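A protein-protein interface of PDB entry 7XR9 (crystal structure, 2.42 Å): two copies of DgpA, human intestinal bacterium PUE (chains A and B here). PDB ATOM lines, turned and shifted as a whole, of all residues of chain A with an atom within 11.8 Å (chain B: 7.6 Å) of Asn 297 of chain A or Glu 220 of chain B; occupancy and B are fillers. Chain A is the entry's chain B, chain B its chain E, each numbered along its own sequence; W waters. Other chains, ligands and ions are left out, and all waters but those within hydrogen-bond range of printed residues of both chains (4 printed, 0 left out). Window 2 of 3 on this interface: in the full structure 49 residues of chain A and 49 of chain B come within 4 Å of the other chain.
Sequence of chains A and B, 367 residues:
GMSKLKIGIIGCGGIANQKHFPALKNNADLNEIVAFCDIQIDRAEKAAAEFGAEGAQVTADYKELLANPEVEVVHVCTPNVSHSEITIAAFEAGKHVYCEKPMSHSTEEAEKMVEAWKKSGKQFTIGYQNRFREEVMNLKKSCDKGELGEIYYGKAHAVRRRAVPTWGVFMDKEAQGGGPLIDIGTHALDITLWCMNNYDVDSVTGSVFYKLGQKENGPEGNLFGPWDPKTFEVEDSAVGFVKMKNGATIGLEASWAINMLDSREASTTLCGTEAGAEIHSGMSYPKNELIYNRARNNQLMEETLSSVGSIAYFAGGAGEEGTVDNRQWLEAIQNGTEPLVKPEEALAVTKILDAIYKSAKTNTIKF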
ATOM      1  N   GLY A 272     -13.289  -7.188  -0.447  1.00  0.00           N
ATOM      2  CA  GLY A 272     -11.989  -7.298   0.175  1.00  0.00           C
ATOM      3  C   GLY A 272     -10.933  -7.744  -0.819  1.00  0.00           C
ATOM      4  O   GLY A 272     -11.235  -8.161  -1.941  1.00  0.00           O
ATOM      5  N   THR A 273      -9.675  -7.655  -0.378  1.00  0.00           N
ATOM      6  CA  THR A 273      -8.547  -8.037  -1.226  1.00  0.00           C
ATOM      7  C   THR A 273      -8.541  -9.529  -1.531  1.00  0.00           C
ATOM      8  O   THR A 273      -7.987  -9.948  -2.550  1.00  0.00           O
ATOM      9  CB  THR A 273      -7.230  -7.641  -0.555  1.00  0.00           C
ATOM     10  OG1 THR A 273      -7.157  -8.241   0.750  1.00  0.00           O
ATOM     11  CG2 THR A 273      -7.141  -6.135  -0.409  1.00  0.00           C
ATOM     12  N   GLU A 274      -9.129 -10.345  -0.657  1.00  0.00           N
ATOM     13  CA  GLU A 274      -9.119 -11.796  -0.811  1.00  0.00           C
ATOM     14  C   GLU A 274     -10.442 -12.358  -1.297  1.00  0.00           C
ATOM     15  O   GLU A 274     -10.450 -13.335  -2.055  1.00  0.00           O
ATOM     16  CB  GLU A 274      -8.768 -12.474   0.521  1.00  0.00           C
ATOM     17  CG  GLU A 274      -7.375 -12.181   1.020  1.00  0.00           C
ATOM     18  CD  GLU A 274      -6.295 -12.705   0.090  1.00  0.00           C
ATOM     19  OE1 GLU A 274      -6.530 -13.708  -0.617  1.00  0.00           O
ATOM     20  OE2 GLU A 274      -5.199 -12.112   0.076  1.00  0.00           O
ATOM     21  N   ALA A 275     -11.554 -11.770  -0.880  1.00  0.00           N
ATOM     22  CA  ALA A 275     -12.867 -12.287  -1.215  1.00  0.00           C
ATOM     23  C   ALA A 275     -13.872 -11.170  -1.014  1.00  0.00           C
ATOM     24  O   ALA A 275     -13.535 -10.076  -0.554  1.00  0.00           O
ATOM     25  CB  ALA A 275     -13.213 -13.512  -0.361  1.00  0.00           C
ATOM     26  N   GLY A 276     -15.121 -11.453  -1.376  1.00  0.00           N
ATOM     27  CA  GLY A 276     -16.205 -10.536  -1.114  1.00  0.00           C
ATOM     28  C   GLY A 276     -17.391 -11.289  -0.548  1.00  0.00           C
ATOM     29  O   GLY A 276     -17.461 -12.519  -0.622  1.00  0.00           O
ATOM     30  N   ASN A 293     -18.118 -14.499  -2.515  1.00  0.00           N
ATOM     31  CA  ASN A 293     -17.608 -14.606  -3.871  1.00  0.00           C
ATOM     32  C   ASN A 293     -16.099 -14.439  -3.835  1.00  0.00           C
ATOM     33  O   ASN A 293     -15.578 -13.459  -3.293  1.00  0.00           O
ATOM     34  CB  ASN A 293     -18.249 -13.567  -4.809  1.00  0.00           C
ATOM     35  CG  ASN A 293     -17.812 -12.155  -4.493  1.00  0.00           C
ATOM     36  OD1 ASN A 293     -16.728 -11.733  -4.886  1.00  0.00           O
ATOM     37  ND2 ASN A 293     -18.649 -11.415  -3.772  1.00  0.00           N
ATOM     38  N   ARG A 294     -15.401 -15.415  -4.401  1.00  0.00           N
ATOM     39  CA  ARG A 294     -13.951 -15.386  -4.459  1.00  0.00           C
ATOM     40  C   ARG A 294     -13.516 -16.081  -5.737  1.00  0.00           C
ATOM     41  O   ARG A 294     -14.317 -16.704  -6.436  1.00  0.00           O
ATOM     42  CB  ARG A 294     -13.334 -16.080  -3.245  1.00  0.00           C
ATOM     43  CG  ARG A 294     -13.745 -17.530  -3.165  1.00  0.00           C
ATOM     44  CD  ARG A 294     -12.803 -18.314  -2.313  1.00  0.00           C
ATOM     45  NE  ARG A 294     -13.378 -19.576  -1.865  1.00  0.00           N
ATOM     46  CZ  ARG A 294     -12.726 -20.436  -1.092  1.00  0.00           C
ATOM     47  NH1 ARG A 294     -11.490 -20.153  -0.697  1.00  0.00           N
ATOM     48  NH2 ARG A 294     -13.306 -21.563  -0.705  1.00  0.00           N
ATOM     49  N   ALA A 295     -12.226 -15.980  -6.020  1.00  0.00           N
ATOM     50  CA  ALA A 295     -11.602 -16.834  -7.014  1.00  0.00           C
ATOM     51  C   ALA A 295     -10.981 -18.028  -6.301  1.00  0.00           C
ATOM     52  O   ALA A 295     -10.199 -17.862  -5.361  1.00  0.00           O
ATOM     53  CB  ALA A 295     -10.547 -16.065  -7.810  1.00  0.00           C
ATOM     54  N   ARG A 296     -11.353 -19.229  -6.732  1.00  0.00           N
ATOM     55  CA  ARG A 296     -10.788 -20.463  -6.209  1.00  0.00           C
ATOM     56  C   ARG A 296     -10.223 -21.267  -7.368  1.00  0.00           C
ATOM     57  O   ARG A 296     -10.936 -21.538  -8.340  1.00  0.00           O
ATOM     58  CB  ARG A 296     -11.844 -21.272  -5.457  1.00  0.00           C
ATOM     59  CG  ARG A 296     -11.293 -22.530  -4.806  1.00  0.00           C
ATOM     60  CD  ARG A 296     -12.373 -23.285  -4.093  1.00  0.00           C
ATOM     61  NE  ARG A 296     -11.860 -24.493  -3.459  1.00  0.00           N
ATOM     62  CZ  ARG A 296     -12.501 -25.147  -2.497  1.00  0.00           C
ATOM     63  NH1 ARG A 296     -13.665 -24.695  -2.067  1.00  0.00           N
ATOM     64  NH2 ARG A 296     -11.977 -26.242  -1.961  1.00  0.00           N
ATOM     65  N   ASN A 297      -8.952 -21.655  -7.265  1.00  0.00           N
ATOM     66  CA  ASN A 297      -8.277 -22.419  -8.322  1.00  0.00           C
ATOM     67  C   ASN A 297      -8.570 -21.828  -9.701  1.00  0.00           C
ATOM     68  O   ASN A 297      -8.967 -22.523 -10.636  1.00  0.00           O
ATOM     69  CB  ASN A 297      -8.668 -23.894  -8.259  1.00  0.00           C
ATOM     70  CG  ASN A 297      -8.449 -24.492  -6.878  1.00  0.00           C
ATOM     71  OD1 ASN A 297      -7.386 -24.326  -6.285  1.00  0.00           O
ATOM     72  ND2 ASN A 297      -9.462 -25.175  -6.356  1.00  0.00           N
ATOM     73  N   ASN A 298      -8.420 -20.502  -9.793  1.00  0.00           N
ATOM     74  CA  ASN A 298      -8.520 -19.754 -11.045  1.00  0.00           C
ATOM     75  C   ASN A 298      -9.932 -19.750 -11.637  1.00  0.00           C
ATOM     76  O   ASN A 298     -10.102 -19.587 -12.847  1.00  0.00           O
ATOM     77  CB  ASN A 298      -7.514 -20.274 -12.073  1.00  0.00           C
ATOM     78  CG  ASN A 298      -7.306 -19.308 -13.198  1.00  0.00           C
ATOM     79  OD1 ASN A 298      -6.944 -18.153 -12.972  1.00  0.00           O
ATOM     80  ND2 ASN A 298      -7.551 -19.760 -14.421  1.00  0.00           N
ATOM     81  N   GLN A 299     -10.962 -19.907 -10.807  1.00  0.00           N
ATOM     82  CA  GLN A 299     -12.334 -19.797 -11.280  1.00  0.00           C
ATOM     83  C   GLN A 299     -13.146 -18.949 -10.310  1.00  0.00           C
ATOM     84  O   GLN A 299     -12.968 -19.042  -9.091  1.00  0.00           O
ATOM     85  CB  GLN A 299     -12.981 -21.174 -11.453  1.00  0.00           C
ATOM     86  CG  GLN A 299     -12.425 -21.970 -12.626  1.00  0.00           C
ATOM     87  CD  GLN A 299     -13.250 -23.196 -12.941  1.00  0.00           C
ATOM     88  OE1 GLN A 299     -13.258 -24.166 -12.186  1.00  0.00           O
ATOM     89  NE2 GLN A 299     -13.980 -23.145 -14.050  1.00  0.00           N
ATOM     90  N   LEU A 300     -14.025 -18.116 -10.865  1.00  0.00           N
ATOM     91  CA  LEU A 300     -14.929 -17.309 -10.055  1.00  0.00           C
ATOM     92  C   LEU A 300     -16.035 -18.188  -9.491  1.00  0.00           C
ATOM     93  O   LEU A 300     -16.792 -18.799 -10.251  1.00  0.00           O
ATOM     94  CB  LEU A 300     -15.528 -16.182 -10.891  1.00  0.00           C
ATOM     95  CG  LEU A 300     -14.574 -15.109 -11.402  1.00  0.00           C
ATOM     96  CD1 LEU A 300     -15.352 -14.063 -12.184  1.00  0.00           C
ATOM     97  CD2 LEU A 300     -13.801 -14.481 -10.243  1.00  0.00           C
ATOM     98  N   MET A 301     -16.134 -18.252  -8.166  1.00  0.00           N
ATOM     99  CA  MET A 301     -17.116 -19.096  -7.500  1.00  0.00           C
ATOM    100  C   MET A 301     -17.934 -18.265  -6.523  1.00  0.00           C
ATOM    101  O   MET A 301     -17.635 -17.097  -6.260  1.00  0.00           O
ATOM    102  CB  MET A 301     -16.445 -20.266  -6.768  1.00  0.00           C
ATOM    103  CG  MET A 301     -15.507 -21.088  -7.645  1.00  0.00           C
ATOM    104  SD  MET A 301     -15.254 -22.741  -6.975  1.00  0.00           S
ATOM    105  CE  MET A 301     -16.688 -23.620  -7.573  1.00  0.00           C
ATOM    106  N   GLU A 302     -18.980 -18.877  -5.982  1.00  0.00           N
ATOM    107  CA  GLU A 302     -19.832 -18.193  -5.020  1.00  0.00           C
ATOM    108  C   GLU A 302     -20.326 -19.214  -4.010  1.00  0.00           C
ATOM    109  O   GLU A 302     -20.754 -20.308  -4.390  1.00  0.00           O
ATOM    110  CB  GLU A 302     -21.006 -17.482  -5.711  1.00  0.00           C
ATOM    111  CG  GLU A 302     -21.704 -18.327  -6.757  1.00  0.00           C
ATOM    112  CD  GLU A 302     -22.599 -17.523  -7.696  1.00  0.00           C
ATOM    113  OE1 GLU A 302     -22.072 -16.758  -8.535  1.00  0.00           O
ATOM    114  OE2 GLU A 302     -23.840 -17.654  -7.586  1.00  0.00           O
ATOM    115  N   GLU A 303     -20.250 -18.859  -2.728  1.00  0.00           N
ATOM    116  CA  GLU A 303     -20.572 -19.770  -1.637  1.00  0.00           C
ATOM    117  C   GLU A 303     -21.837 -19.281  -0.951  1.00  0.00           C
ATOM    118  O   GLU A 303     -21.830 -18.243  -0.276  1.00  0.00           O
ATOM    119  CB  GLU A 303     -19.423 -19.872  -0.644  1.00  0.00           C
ATOM    120  CG  GLU A 303     -19.670 -20.887   0.464  1.00  0.00           C
ATOM    121  CD  GLU A 303     -18.384 -21.341   1.131  1.00  0.00           C
ATOM    122  OE1 GLU A 303     -17.342 -20.667   0.952  1.00  0.00           O
ATOM    123  OE2 GLU A 303     -18.415 -22.377   1.827  1.00  0.00           O
ATOM    124  N   ARG B 161     -16.893  -8.013 -12.111  1.00  0.00           N
ATOM    125  CA  ARG B 161     -16.307  -8.786 -11.022  1.00  0.00           C
ATOM    126  C   ARG B 161     -14.829  -9.085 -11.287  1.00  0.00           C
ATOM    127  O   ARG B 161     -13.956  -8.746 -10.479  1.00  0.00           O
ATOM    128  CB  ARG B 161     -17.106 -10.073 -10.812  1.00  0.00           C
ATOM    129  CG  ARG B 161     -16.440 -11.012  -9.838  1.00  0.00           C
ATOM    130  CD  ARG B 161     -17.405 -12.030  -9.315  1.00  0.00           C
ATOM    131  NE  ARG B 161     -16.723 -12.965  -8.435  1.00  0.00           N
ATOM    132  CZ  ARG B 161     -17.166 -14.184  -8.173  1.00  0.00           C
ATOM    133  NH1 ARG B 161     -18.302 -14.598  -8.723  1.00  0.00           N
ATOM    134  NH2 ARG B 161     -16.473 -14.981  -7.368  1.00  0.00           N
ATOM    135  N   ARG B 162     -14.526  -9.737 -12.412  1.00  0.00           N
ATOM    136  CA  ARG B 162     -13.134  -9.900 -12.856  1.00  0.00           C
ATOM    137  C   ARG B 162     -13.151 -10.041 -14.377  1.00  0.00           C
ATOM    138  O   ARG B 162     -13.299 -11.146 -14.906  1.00  0.00           O
ATOM    139  CB  ARG B 162     -12.448 -11.087 -12.200  1.00  0.00           C
ATOM    140  CG  ARG B 162     -10.929 -11.127 -12.425  1.00  0.00           C
ATOM    141  CD  ARG B 162     -10.190 -11.294 -11.109  1.00  0.00           C
ATOM    142  NE  ARG B 162     -10.856 -10.526 -10.069  1.00  0.00           N
ATOM    143  CZ  ARG B 162     -11.061 -10.951  -8.831  1.00  0.00           C
ATOM    144  NH1 ARG B 162     -10.636 -12.151  -8.461  1.00  0.00           N
ATOM    145  NH2 ARG B 162     -11.693 -10.169  -7.965  1.00  0.00           N
ATOM    146  N   LEU B 212      -6.698  -5.170  -6.127  1.00  0.00           N
ATOM    147  CA  LEU B 212      -6.412  -6.414  -6.824  1.00  0.00           C
ATOM    148  C   LEU B 212      -5.481  -6.215  -8.001  1.00  0.00           C
ATOM    149  O   LEU B 212      -4.947  -7.202  -8.515  1.00  0.00           O
ATOM    150  CB  LEU B 212      -7.708  -7.068  -7.310  1.00  0.00           C
ATOM    151  CG  LEU B 212      -8.887  -7.011  -6.337  1.00  0.00           C
ATOM    152  CD1 LEU B 212     -10.061  -7.800  -6.883  1.00  0.00           C
ATOM    153  CD2 LEU B 212      -8.479  -7.529  -4.976  1.00  0.00           C
ATOM    154  N   LYS B 215      -1.948  -7.214  -7.212  1.00  0.00           N
ATOM    155  CA  LYS B 215      -1.983  -8.321  -6.271  1.00  0.00           C
ATOM    156  C   LYS B 215      -1.650  -9.608  -7.015  1.00  0.00           C
ATOM    157  O   LYS B 215      -2.149  -9.839  -8.122  1.00  0.00           O
ATOM    158  CB  LYS B 215      -3.363  -8.398  -5.619  1.00  0.00           C
ATOM    159  CG  LYS B 215      -3.407  -9.121  -4.305  1.00  0.00           C
ATOM    160  CD  LYS B 215      -4.787  -9.003  -3.678  1.00  0.00           C
ATOM    161  CE  LYS B 215      -5.086 -10.187  -2.773  1.00  0.00           C
ATOM    162  NZ  LYS B 215      -3.876 -10.612  -2.039  1.00  0.00           N
ATOM    163  N   GLU B 216      -0.802 -10.443  -6.414  1.00  0.00           N
ATOM    164  CA  GLU B 216      -0.295 -11.601  -7.143  1.00  0.00           C
ATOM    165  C   GLU B 216      -1.428 -12.522  -7.578  1.00  0.00           C
ATOM    166  O   GLU B 216      -1.521 -12.891  -8.755  1.00  0.00           O
ATOM    167  CB  GLU B 216       0.725 -12.353  -6.291  1.00  0.00           C
ATOM    168  CG  GLU B 216       1.606 -13.283  -7.092  1.00  0.00           C
ATOM    169  CD  GLU B 216       1.918 -14.560  -6.347  1.00  0.00           C
ATOM    170  OE1 GLU B 216       1.103 -15.505  -6.424  1.00  0.00           O
ATOM    171  OE2 GLU B 216       2.981 -14.619  -5.692  1.00  0.00           O
ATOM    172  N   ASN B 217      -2.304 -12.894  -6.650  1.00  0.00           N
ATOM    173  CA  ASN B 217      -3.466 -13.707  -6.988  1.00  0.00           C
ATOM    174  C   ASN B 217      -4.538 -12.924  -7.739  1.00  0.00           C
ATOM    175  O   ASN B 217      -5.456 -13.540  -8.289  1.00  0.00           O
ATOM    176  CB  ASN B 217      -4.064 -14.284  -5.709  1.00  0.00           C
ATOM    177  CG  ASN B 217      -4.157 -13.245  -4.613  1.00  0.00           C
ATOM    178  OD1 ASN B 217      -5.173 -12.561  -4.478  1.00  0.00           O
ATOM    179  ND2 ASN B 217      -3.078 -13.094  -3.846  1.00  0.00           N
ATOM    180  N   GLY B 218      -4.441 -11.595  -7.761  1.00  0.00           N
ATOM    181  CA  GLY B 218      -5.422 -10.733  -8.374  1.00  0.00           C
ATOM    182  C   GLY B 218      -6.013 -11.221  -9.685  1.00  0.00           C
ATOM    183  O   GLY B 218      -7.236 -11.267  -9.847  1.00  0.00           O
ATOM    184  N   PRO B 219      -5.168 -11.559 -10.663  1.00  0.00           N
ATOM    185  CA  PRO B 219      -5.696 -11.996 -11.967  1.00  0.00           C
ATOM    186  C   PRO B 219      -6.432 -13.333 -11.943  1.00  0.00           C
ATOM    187  O   PRO B 219      -7.048 -13.690 -12.964  1.00  0.00           O
ATOM    188  CB  PRO B 219      -4.439 -12.075 -12.841  1.00  0.00           C
ATOM    189  CG  PRO B 219      -3.486 -11.128 -12.205  1.00  0.00           C
ATOM    190  CD  PRO B 219      -3.734 -11.230 -10.741  1.00  0.00           C
ATOM    191  N   GLU B 220      -6.378 -14.083 -10.839  1.00  0.00           N
ATOM    192  CA  GLU B 220      -7.057 -15.371 -10.758  1.00  0.00           C
ATOM    193  C   GLU B 220      -8.512 -15.233 -11.170  1.00  0.00           C
ATOM    194  O   GLU B 220      -9.269 -14.462 -10.569  1.00  0.00           O
ATOM    195  CB  GLU B 220      -6.977 -15.931  -9.335  1.00  0.00           C
ATOM    196  CG  GLU B 220      -5.887 -16.960  -9.094  1.00  0.00           C
ATOM    197  CD  GLU B 220      -6.154 -17.784  -7.842  1.00  0.00           C
ATOM    198  OE1 GLU B 220      -7.065 -18.645  -7.877  1.00  0.00           O
ATOM    199  OE2 GLU B 220      -5.472 -17.553  -6.816  1.00  0.00           O
ATOM    200  N   GLY B 221      -8.895 -15.977 -12.199  1.00  0.00           N
ATOM    201  CA  GLY B 221     -10.271 -16.008 -12.640  1.00  0.00           C
ATOM    202  C   GLY B 221     -10.694 -14.893 -13.572  1.00  0.00           C
ATOM    203  O   GLY B 221     -11.899 -14.718 -13.780  1.00  0.00           O
ATOM    204  N   ASN B 222      -9.760 -14.140 -14.148  1.00  0.00           N
ATOM    205  CA  ASN B 222     -10.162 -13.047 -15.024  1.00  0.00           C
ATOM    206  C   ASN B 222     -10.723 -13.594 -16.326  1.00  0.00           C
ATOM    207  O   ASN B 222     -10.117 -14.459 -16.967  1.00  0.00           O
ATOM    208  CB  ASN B 222      -8.999 -12.104 -15.310  1.00  0.00           C
ATOM    209  CG  ASN B 222      -9.453 -10.815 -15.980  1.00  0.00           C
ATOM    210  OD1 ASN B 222     -10.263 -10.067 -15.426  1.00  0.00           O
ATOM    211  ND2 ASN B 222      -8.938 -10.552 -17.177  1.00  0.00           N
ATOM    212  N   LEU B 223     -11.888 -13.075 -16.711  1.00  0.00           N
ATOM    213  CA  LEU B 223     -12.584 -13.496 -17.921  1.00  0.00           C
ATOM    214  C   LEU B 223     -11.646 -13.586 -19.119  1.00  0.00           C
ATOM    215  O   LEU B 223     -11.734 -14.524 -19.921  1.00  0.00           O
ATOM    216  CB  LEU B 223     -13.718 -12.520 -18.214  1.00  0.00           C
ATOM    217  CG  LEU B 223     -14.597 -12.866 -19.410  1.00  0.00           C
ATOM    218  CD1 LEU B 223     -15.250 -14.214 -19.195  1.00  0.00           C
ATOM    219  CD2 LEU B 223     -15.633 -11.797 -19.601  1.00  0.00           C
ATOM    220  N   GLY B 225      -8.331 -13.740 -19.189  1.00  0.00           N
ATOM    221  CA  GLY B 225      -7.056 -14.373 -18.958  1.00  0.00           C
ATOM    222  C   GLY B 225      -6.166 -13.566 -18.038  1.00  0.00           C
ATOM    223  O   GLY B 225      -6.553 -12.511 -17.519  1.00  0.00           O
ATOM    224  N   PRO B 226      -4.946 -14.045 -17.824  1.00  0.00           N
ATOM    225  CA  PRO B 226      -4.059 -13.376 -16.877  1.00  0.00           C
ATOM    226  C   PRO B 226      -3.610 -12.026 -17.397  1.00  0.00           C
ATOM    227  O   PRO B 226      -3.494 -11.795 -18.602  1.00  0.00           O
ATOM    228  CB  PRO B 226      -2.869 -14.338 -16.752  1.00  0.00           C
ATOM    229  CG  PRO B 226      -3.321 -15.622 -17.394  1.00  0.00           C
ATOM    230  CD  PRO B 226      -4.304 -15.215 -18.437  1.00  0.00           C
ATOM    231  N   TRP B 227      -3.390 -11.124 -16.456  1.00  0.00           N
ATOM    232  CA  TRP B 227      -2.612  -9.919 -16.669  1.00  0.00           C
ATOM    233  C   TRP B 227      -1.450  -9.947 -15.684  1.00  0.00           C
ATOM    234  O   TRP B 227      -1.448 -10.722 -14.725  1.00  0.00           O
ATOM    235  CB  TRP B 227      -3.479  -8.658 -16.509  1.00  0.00           C
ATOM    236  CG  TRP B 227      -4.547  -8.758 -15.459  1.00  0.00           C
ATOM    237  CD1 TRP B 227      -5.815  -9.257 -15.602  1.00  0.00           C
ATOM    238  CD2 TRP B 227      -4.435  -8.343 -14.113  1.00  0.00           C
ATOM    239  NE1 TRP B 227      -6.503  -9.169 -14.411  1.00  0.00           N
ATOM    240  CE2 TRP B 227      -5.672  -8.609 -13.479  1.00  0.00           C
ATOM    241  CE3 TRP B 227      -3.415  -7.771 -13.379  1.00  0.00           C
ATOM    242  CZ2 TRP B 227      -5.899  -8.322 -12.157  1.00  0.00           C
ATOM    243  CZ3 TRP B 227      -3.635  -7.504 -12.094  1.00  0.00           C
ATOM    244  CH2 TRP B 227      -4.866  -7.761 -11.478  1.00  0.00           C
ATOM    245  N   ASN B 259     -14.315  -7.878  -5.795  1.00  0.00           N
ATOM    246  CA  ASN B 259     -14.922  -9.095  -5.258  1.00  0.00           C
ATOM    247  C   ASN B 259     -16.373  -8.806  -4.878  1.00  0.00           C
ATOM    248  O   ASN B 259     -16.800  -8.893  -3.728  1.00  0.00           O
ATOM    249  CB  ASN B 259     -14.093  -9.631  -4.102  1.00  0.00           C
ATOM    250  CG  ASN B 259     -12.812 -10.280  -4.591  1.00  0.00           C
ATOM    251  OD1 ASN B 259     -12.825 -10.983  -5.602  1.00  0.00           O
ATOM    252  ND2 ASN B 259     -11.696 -10.028  -3.901  1.00  0.00           N
HETATM  253  O   HOH W   1     -14.627 -13.047  -6.517  1.00  0.00           O
HETATM  254  O   HOH W   2      -8.870 -11.652  -4.408  1.00  0.00           O
HETATM  255  O   HOH W   3     -12.911  -6.503  -3.874  1.00  0.00           O
HETATM  256  O   HOH W   4      -7.426 -20.322  -4.875  1.00  0.00           O
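No position is printed for both chains.
Among the printed residues, merely in contact across the chains: Thr 273 of chain A with Lys 215 of chain B (2.9 Å), Gly 276 of chain A with Asn 259 of chain B (3.1 Å), Asn 293 of chain A with Arg 161 of chain B (3.4 Å), Ala 295 of chain A with Glu 220 of chain B (3.4 Å), Thr 273 of chain A with Leu 212 of chain B (3.5 Å), Leu 300 of chain A with Gly 221 of chain B (3.6 Å), Asn 297 of chain A with Glu 220 of chain B (3.6 Å), Glu 274 of chain A with Asn 259 of chain B (3.7 Å), Leu 300 of chain A with Arg 161 of chain B (3.8 Å), Thr 273 of chain A with Asn 259 of chain B (3.9 Å) and Ala 295 of chain A with Arg 162 of chain B (3.97 Å).
O of Gly 272 of chain A is in hydrogen-bond range of ND2 of Asn 259 of chain B (2.7 Å). The side-chain carboxylate of Glu 274 of chain A lies within salt-bridge range of the side-chain amino group of Lys 215 of chain B, at 2.9 Å. N of Ala 275 of chain A sits close to ND2 of Asn 259 of chain B. O of Asn 259 of chain B sits close to OD1 of Asn 293 of chain A (3.1 Å). The backbone carbonyl oxygen (O) of Arg 294 of chain A lies within hydrogen-bond range of the guanidinium group (NH2) of Arg 161 of chain B. N of Asn 298 of chain A lies within hydrogen-bond range of OE1 of Glu 220 of chain B (3.0 Å). The side-chain amide oxygen (OD1) of Asn 298 of chain A is in hydrogen-bond range of the backbone NH (N) of Gly 221 of chain B (3.0 Å). O of Met 301 of chain A is in hydrogen-bond range of NH2 of Arg 161 of chain B, at 2.7 Å.
Water W2 lies within hydrogen-bond range of O of Thr 273 of chain A (2.7 Å), O of Glu 274 of chain A (3.3 Å) and ND2 of Asn 259 of chain B (3.3 Å). Water W3 lies within hydrogen-bond range of the backbone NH (N) of Asn 259 of chain B (2.7 Å) and the backbone carbonyl oxygen (O) of Gly 272 of chain A (3.0 Å). Water W1 lies within hydrogen-bond range of NH2 of Arg 161 of chain B (2.8 Å), OD1 of Asn 259 of chain B (2.9 Å), OD1 of Asn 293 of chain A (3.0 Å) and N of Arg 294 of chain A (3.3 Å). Water W4 bridges N of Asn 297 of chain A (3.1 Å) and OE1 of Glu 220 of chain B (3.5 Å).
Printed residues of chain B within 4 Å of Asn 293 of chain A: Arg 161 (3.4 Å) and Asn 259 (2.9 Å). Printed residues of chain B within 4 Å of Leu 300 of chain A: Arg 161 and Gly 221. Of the printed residues of chain A, Arg 161 of chain B touches Asn 293 (3.4 Å), Arg 294 (2.9 Å), Leu 300 (3.8 Å) and Met 301 (2.7 Å). Printed residues of chain A within 4 Å of Leu 212 of chain B: Thr 273 (3.5 Å). Pro 219 of chain B touches none of the printed residues of chain A. Glu 220 of chain B touches three residues of chain A. Of chain A, only Asn 298 (3.0 Å) and Leu 300 (3.6 Å) come within 4 Å of Gly 221 of chain B. Asn 222 of chain B touches none of the printed residues of chain A. Pro 226 of chain B touches none of the printed residues of chain A. The nearest residue of chain A that does not touch Glu 220 of chain B is Arg 296 of chain A (4.1 Å).
Of the 16 printed residues of chain B, 7 touch a printed residue of chain A. Hydrophobic or aromatic side chains of chain B that line the printed part of chain A: Leu 212. Of the 16 printed residues of chain A, 12 touch a printed residue of chain B. Along chain A the printed residues that touch a printed residue of chain B span positions 272 to 301. Among the printed residues, 19 pairs touch across the chains.
N of Met 301 of chain A sits at hydrogen-bond distance from O of Arg 294 of chain A (2.9 Å). NH1 of Arg 162 of chain B sits close to O of Glu 220 of chain B. The side-chain amide oxygen (OD1) of Asn 222 of chain B sits close to the backbone carbonyl oxygen (O) of Arg 162 of chain B (3.3 Å). O of Arg 162 of chain B is in hydrogen-bond range of N of Leu 223 of chain B. NH2 of Arg 162 of chain B is in hydrogen-bond range of OD1 of Asn 259 of chain B (2.7 Å). ND2 of Asn 217 of chain B sits close to NZ of Lys 215 of chain B (3.2 Å).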
